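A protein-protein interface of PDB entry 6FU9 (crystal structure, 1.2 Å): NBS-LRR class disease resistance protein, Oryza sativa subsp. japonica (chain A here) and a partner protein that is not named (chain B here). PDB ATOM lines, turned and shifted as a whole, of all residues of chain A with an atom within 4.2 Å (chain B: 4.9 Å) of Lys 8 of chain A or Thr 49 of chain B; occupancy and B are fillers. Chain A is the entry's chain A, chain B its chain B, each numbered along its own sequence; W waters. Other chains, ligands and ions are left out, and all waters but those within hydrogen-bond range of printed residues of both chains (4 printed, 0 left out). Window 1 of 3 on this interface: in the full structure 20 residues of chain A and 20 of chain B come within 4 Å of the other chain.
NZ of Lys 8 of chain A is in hydrogen-bond range of O of Thr 49 of chain B, at 3.4 Å.
The backbone carbonyl oxygen (O) of Ser 76 of chain A lies within hydrogen-bond range of the backbone NH (N) of Lys 8 of chain A (2.8 Å).
NE1 of Trp 36 of chain B lies within hydrogen-bond range of O of Thr 49 of chain B, at 3.4 Å.
Of the 8 printed residues of chain A, 1 touches a printed residue of chain B.
Water W1 lies within hydrogen-bond range of OE1 of Glu 74 of chain A (2.5 Å), O of Thr 49 of chain B (2.7 Å) and NE1 of Trp 36 of chain B (2.9 Å).
Water W2 lies within hydrogen-bond range of OG1 of Thr 49 of chain B (2.7 Å) and NZ of Lys 8 of chain A (2.9 Å).
Water W4 lies within hydrogen-bond range of OE2 of Glu 74 of chain A, NZ of Lys 8 of chain A and O of Thr 49 of chain B.
Water W3 lies within hydrogen-bond range of the side-chain amino group (NZ) of Lys 8 of chain A (3.0 Å) and the side-chain hydroxyl (OH) of Tyr 51 of chain B (3.1 Å).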
ATOM      1  N   GLN A   7     -27.908   9.931  19.445  1.00  0.00           N
ATOM      2  CA  GLN A   7     -27.503   9.594  20.788  1.00  0.00           C
ATOM      3  C   GLN A   7     -26.475   8.432  20.772  1.00  0.00           C
ATOM      4  O   GLN A   7     -26.569   7.590  19.883  1.00  0.00           O
ATOM      5  CB  GLN A   7     -28.716   8.961  21.543  1.00  0.00           C
ATOM      6  CG  GLN A   7     -29.909   9.793  21.959  1.00  0.00           C
ATOM      7  CD  GLN A   7     -31.067   8.844  22.257  1.00  0.00           C
ATOM      8  OE1 GLN A   7     -31.700   8.320  21.412  1.00  0.00           O
ATOM      9  NE2 GLN A   7     -31.408   8.762  23.529  1.00  0.00           N
ATOM     10  N   LYS A   8     -25.617   8.412  21.759  1.00  0.00           N
ATOM     11  CA  LYS A   8     -24.696   7.303  22.047  1.00  0.00           C
ATOM     12  C   LYS A   8     -24.835   6.918  23.455  1.00  0.00           C
ATOM     13  O   LYS A   8     -24.643   7.763  24.384  1.00  0.00           O
ATOM     14  CB  LYS A   8     -23.268   7.722  21.739  1.00  0.00           C
ATOM     15  CG  LYS A   8     -22.252   6.614  21.946  1.00  0.00           C
ATOM     16  CD  LYS A   8     -20.865   7.091  21.494  1.00  0.00           C
ATOM     17  CE  LYS A   8     -19.779   6.129  21.712  1.00  0.00           C
ATOM     18  NZ  LYS A   8     -18.569   6.798  21.202  1.00  0.00           N
ATOM     19  N   ILE A   9     -25.228   5.662  23.742  1.00  0.00           N
ATOM     20  CA  ILE A   9     -25.437   5.160  25.059  1.00  0.00           C
ATOM     21  C   ILE A   9     -24.544   3.933  25.229  1.00  0.00           C
ATOM     22  O   ILE A   9     -24.576   3.029  24.385  1.00  0.00           O
ATOM     23  CB  ILE A   9     -26.869   4.716  25.302  1.00  0.00           C
ATOM     24  CG1 ILE A   9     -27.872   5.857  25.011  1.00  0.00           C
ATOM     25  CG2 ILE A   9     -27.028   4.218  26.714  1.00  0.00           C
ATOM     26  CD1 ILE A   9     -29.283   5.424  24.865  1.00  0.00           C
ATOM     27  N   VAL A  48     -22.302  -0.761  23.190  1.00  0.00           N
ATOM     28  CA  VAL A  48     -22.328   0.593  22.646  1.00  0.00           C
ATOM     29  C   VAL A  48     -23.492   0.685  21.679  1.00  0.00           C
ATOM     30  O   VAL A  48     -23.542  -0.034  20.677  1.00  0.00           O
ATOM     31  CB  VAL A  48     -20.989   0.978  21.977  1.00  0.00           C
ATOM     32  CG1 VAL A  48     -21.114   2.434  21.471  1.00  0.00           C
ATOM     33  CG2 VAL A  48     -19.804   0.783  22.858  1.00  0.00           C
ATOM     34  N   VAL A  49     -24.414   1.614  21.965  1.00  0.00           N
ATOM     35  CA  VAL A  49     -25.657   1.784  21.264  1.00  0.00           C
ATOM     36  C   VAL A  49     -25.752   3.143  20.622  1.00  0.00           C
ATOM     37  O   VAL A  49     -25.520   4.147  21.321  1.00  0.00           O
ATOM     38  CB  VAL A  49     -26.840   1.549  22.190  1.00  0.00           C
ATOM     39  CG1 VAL A  49     -28.131   1.507  21.411  1.00  0.00           C
ATOM     40  CG2 VAL A  49     -26.639   0.311  23.068  1.00  0.00           C
ATOM     41  N   GLU A  74     -22.006   5.453  29.872  1.00  0.00           N
ATOM     42  CA  GLU A  74     -21.924   6.749  29.213  1.00  0.00           C
ATOM     43  C   GLU A  74     -23.230   7.103  28.551  1.00  0.00           C
ATOM     44  O   GLU A  74     -23.929   6.246  27.982  1.00  0.00           O
ATOM     45  CB  GLU A  74     -20.833   6.684  28.132  1.00  0.00           C
ATOM     46  CG  GLU A  74     -20.792   7.902  27.229  1.00  0.00           C
ATOM     47  CD  GLU A  74     -19.800   7.732  26.111  1.00  0.00           C
ATOM     48  OE1 GLU A  74     -18.904   6.887  26.198  1.00  0.00           O
ATOM     49  OE2 GLU A  74     -19.903   8.528  25.118  1.00  0.00           O
ATOM     50  N   VAL A  75     -23.534   8.406  28.619  1.00  0.00           N
ATOM     51  CA  VAL A  75     -24.606   8.974  27.803  1.00  0.00           C
ATOM     52  C   VAL A  75     -24.023  10.207  27.103  1.00  0.00           C
ATOM     53  O   VAL A  75     -23.493  11.097  27.786  1.00  0.00           O
ATOM     54  CB  VAL A  75     -25.832   9.364  28.672  1.00  0.00           C
ATOM     55  CG1 VAL A  75     -26.891  10.029  27.863  1.00  0.00           C
ATOM     56  CG2 VAL A  75     -26.401   8.142  29.385  1.00  0.00           C
ATOM     57  N   SER A  76     -24.098  10.260  25.785  1.00  0.00           N
ATOM     58  CA  SER A  76     -23.562  11.377  25.049  1.00  0.00           C
ATOM     59  C   SER A  76     -24.338  11.541  23.741  1.00  0.00           C
ATOM     60  O   SER A  76     -25.146  10.692  23.380  1.00  0.00           O
ATOM     61  CB  SER A  76     -22.082  11.224  24.808  1.00  0.00           C
ATOM     62  OG  SER A  76     -21.806  10.088  24.015  1.00  0.00           O
ATOM     63  N   PHE B  23     -12.457  -1.304  20.190  1.00  0.00           N
ATOM     64  CA  PHE B  23     -13.504  -0.390  19.741  1.00  0.00           C
ATOM     65  C   PHE B  23     -14.171  -0.926  18.490  1.00  0.00           C
ATOM     66  O   PHE B  23     -13.659  -1.840  17.818  1.00  0.00           O
ATOM     67  CB  PHE B  23     -12.900   0.984  19.493  1.00  0.00           C
ATOM     68  CG  PHE B  23     -11.894   1.016  18.404  1.00  0.00           C
ATOM     69  CD1 PHE B  23     -10.555   0.775  18.663  1.00  0.00           C
ATOM     70  CD2 PHE B  23     -12.284   1.097  17.101  1.00  0.00           C
ATOM     71  CE1 PHE B  23      -9.654   0.766  17.630  1.00  0.00           C
ATOM     72  CE2 PHE B  23     -11.367   1.073  16.072  1.00  0.00           C
ATOM     73  CZ  PHE B  23     -10.050   0.919  16.346  1.00  0.00           C
ATOM     74  N   ASP B  25     -16.019   1.156  15.232  1.00  0.00           N
ATOM     75  CA  ASP B  25     -16.492   2.443  14.620  1.00  0.00           C
ATOM     76  C   ASP B  25     -17.838   2.215  13.915  1.00  0.00           C
ATOM     77  O   ASP B  25     -17.920   1.560  12.902  1.00  0.00           O
ATOM     78  CB  ASP B  25     -15.448   2.982  13.617  1.00  0.00           C
ATOM     79  CG  ASP B  25     -14.176   3.522  14.309  1.00  0.00           C
ATOM     80  OD1 ASP B  25     -14.279   4.128  15.409  1.00  0.00           O
ATOM     81  OD2 ASP B  25     -13.089   3.292  13.777  1.00  0.00           O
ATOM     82  N   PRO B  32     -15.001   8.701  15.667  1.00  0.00           N
ATOM     83  CA  PRO B  32     -14.498   9.552  16.772  1.00  0.00           C
ATOM     84  C   PRO B  32     -12.968   9.632  16.746  1.00  0.00           C
ATOM     85  O   PRO B  32     -12.268   8.669  16.448  1.00  0.00           O
ATOM     86  CB  PRO B  32     -15.031   8.826  18.029  1.00  0.00           C
ATOM     87  CG  PRO B  32     -15.187   7.402  17.568  1.00  0.00           C
ATOM     88  CD  PRO B  32     -15.672   7.523  16.154  1.00  0.00           C
ATOM     89  N   CYS B  34     -10.710  10.317  19.204  1.00  0.00           N
ATOM     90  CA  CYS B  34      -9.938  10.052  20.397  1.00  0.00           C
ATOM     91  C   CYS B  34     -10.117   8.660  20.942  1.00  0.00           C
ATOM     92  O   CYS B  34     -11.169   8.070  20.844  1.00  0.00           O
ATOM     93  CB  CYS B  34     -10.376  10.995  21.515  1.00  0.00           C
ATOM     94  SG  CYS B  34     -10.499  12.757  21.146  1.00  0.00           S
ATOM     95  N   PHE B  35      -9.044   8.186  21.570  1.00  0.00           N
ATOM     96  CA  PHE B  35      -9.098   7.080  22.495  1.00  0.00           C
ATOM     97  C   PHE B  35      -9.105   7.609  23.917  1.00  0.00           C
ATOM     98  O   PHE B  35      -8.375   8.554  24.232  1.00  0.00           O
ATOM     99  CB  PHE B  35      -7.854   6.167  22.344  1.00  0.00           C
ATOM    100  CG  PHE B  35      -7.774   5.368  21.045  1.00  0.00           C
ATOM    101  CD1 PHE B  35      -8.887   4.843  20.456  1.00  0.00           C
ATOM    102  CD2 PHE B  35      -6.517   5.074  20.511  1.00  0.00           C
ATOM    103  CE1 PHE B  35      -8.757   4.010  19.335  1.00  0.00           C
ATOM    104  CE2 PHE B  35      -6.417   4.309  19.362  1.00  0.00           C
ATOM    105  CZ  PHE B  35      -7.514   3.759  18.828  1.00  0.00           C
ATOM    106  N   TRP B  36      -9.929   6.987  24.760  1.00  0.00           N
ATOM    107  CA  TRP B  36      -9.923   7.265  26.189  1.00  0.00           C
ATOM    108  C   TRP B  36      -9.566   6.040  26.970  1.00  0.00           C
ATOM    109  O   TRP B  36      -9.868   4.911  26.532  1.00  0.00           O
ATOM    110  CB  TRP B  36     -11.273   7.863  26.731  1.00  0.00           C
ATOM    111  CG  TRP B  36     -12.483   6.984  26.604  1.00  0.00           C
ATOM    112  CD1 TRP B  36     -13.437   7.109  25.619  1.00  0.00           C
ATOM    113  CD2 TRP B  36     -12.934   5.952  27.457  1.00  0.00           C
ATOM    114  NE1 TRP B  36     -14.422   6.184  25.817  1.00  0.00           N
ATOM    115  CE2 TRP B  36     -14.131   5.455  26.938  1.00  0.00           C
ATOM    116  CE3 TRP B  36     -12.417   5.348  28.612  1.00  0.00           C
ATOM    117  CZ2 TRP B  36     -14.842   4.400  27.521  1.00  0.00           C
ATOM    118  CZ3 TRP B  36     -13.127   4.339  29.170  1.00  0.00           C
ATOM    119  CH2 TRP B  36     -14.272   3.831  28.618  1.00  0.00           C
ATOM    120  N   ALA B  47     -11.381   1.159  28.379  1.00  0.00           N
ATOM    121  CA  ALA B  47     -10.964   2.113  27.380  1.00  0.00           C
ATOM    122  C   ALA B  47     -11.974   2.136  26.270  1.00  0.00           C
ATOM    123  O   ALA B  47     -12.718   1.166  26.048  1.00  0.00           O
ATOM    124  CB  ALA B  47      -9.558   1.732  26.847  1.00  0.00           C
ATOM    125  N   GLY B  48     -12.020   3.236  25.518  1.00  0.00           N
ATOM    126  CA  GLY B  48     -12.989   3.390  24.440  1.00  0.00           C
ATOM    127  C   GLY B  48     -12.604   4.479  23.486  1.00  0.00           C
ATOM    128  O   GLY B  48     -11.471   4.937  23.449  1.00  0.00           O
ATOM    129  N   THR B  49     -13.584   4.929  22.702  1.00  0.00           N
ATOM    130  CA  THR B  49     -13.417   6.022  21.759  1.00  0.00           C
ATOM    131  C   THR B  49     -14.389   7.150  22.077  1.00  0.00           C
ATOM    132  O   THR B  49     -15.455   6.924  22.618  1.00  0.00           O
ATOM    133  CB  THR B  49     -13.597   5.545  20.289  1.00  0.00           C
ATOM    134  OG1 THR B  49     -14.915   5.067  20.115  1.00  0.00           O
ATOM    135  CG2 THR B  49     -12.587   4.535  19.867  1.00  0.00           C
ATOM    136  N   CYS B  50     -13.963   8.383  21.758  1.00  0.00           N
ATOM    137  CA  CYS B  50     -14.855   9.544  21.953  1.00  0.00           C
ATOM    138  C   CYS B  50     -14.448  10.640  21.005  1.00  0.00           C
ATOM    139  O   CYS B  50     -13.358  10.637  20.425  1.00  0.00           O
ATOM    140  CB  CYS B  50     -14.849  10.060  23.400  1.00  0.00           C
ATOM    141  SG  CYS B  50     -13.265  10.667  24.004  1.00  0.00           S
ATOM    142  N   TYR B  51     -15.354  11.605  20.819  1.00  0.00           N
ATOM    143  CA  TYR B  51     -15.081  12.704  19.930  1.00  0.00           C
ATOM    144  C   TYR B  51     -14.201  13.755  20.554  1.00  0.00           C
ATOM    145  O   TYR B  51     -14.308  14.004  21.744  1.00  0.00           O
ATOM    146  CB  TYR B  51     -16.405  13.367  19.455  1.00  0.00           C
ATOM    147  CG  TYR B  51     -17.247  12.454  18.595  1.00  0.00           C
ATOM    148  CD1 TYR B  51     -16.871  12.173  17.242  1.00  0.00           C
ATOM    149  CD2 TYR B  51     -18.332  11.790  19.066  1.00  0.00           C
ATOM    150  CE1 TYR B  51     -17.570  11.285  16.480  1.00  0.00           C
ATOM    151  CE2 TYR B  51     -19.058  10.877  18.297  1.00  0.00           C
ATOM    152  CZ  TYR B  51     -18.633  10.587  16.988  1.00  0.00           C
ATOM    153  OH  TYR B  51     -19.321   9.662  16.280  1.00  0.00           O
ATOM    154  N   ARG B  90      -6.253   9.437  18.056  1.00  0.00           N
ATOM    155  CA  ARG B  90      -6.047   8.250  17.250  1.00  0.00           C
ATOM    156  C   ARG B  90      -5.092   8.557  16.086  1.00  0.00           C
ATOM    157  O   ARG B  90      -5.007   9.690  15.634  1.00  0.00           O
ATOM    158  CB  ARG B  90      -7.376   7.713  16.750  1.00  0.00           C
ATOM    159  CG  ARG B  90      -8.313   7.261  17.821  1.00  0.00           C
ATOM    160  CD  ARG B  90      -9.699   6.933  17.340  1.00  0.00           C
ATOM    161  NE  ARG B  90      -9.705   5.826  16.361  1.00  0.00           N
ATOM    162  CZ  ARG B  90     -10.814   5.254  15.927  1.00  0.00           C
ATOM    163  NH1 ARG B  90     -12.009   5.782  16.215  1.00  0.00           N
ATOM    164  NH2 ARG B  90     -10.766   4.198  15.131  1.00  0.00           N
HETATM  165  O   HOH W   1     -17.072   6.110  24.634  1.00  0.00           O
HETATM  166  O   HOH W   2     -17.231   4.279  21.172  1.00  0.00           O
HETATM  167  O   HOH W   3     -18.817   7.291  18.256  1.00  0.00           O
HETATM  168  O   HOH W   4     -18.041   8.626  23.160  1.00  0.00           O
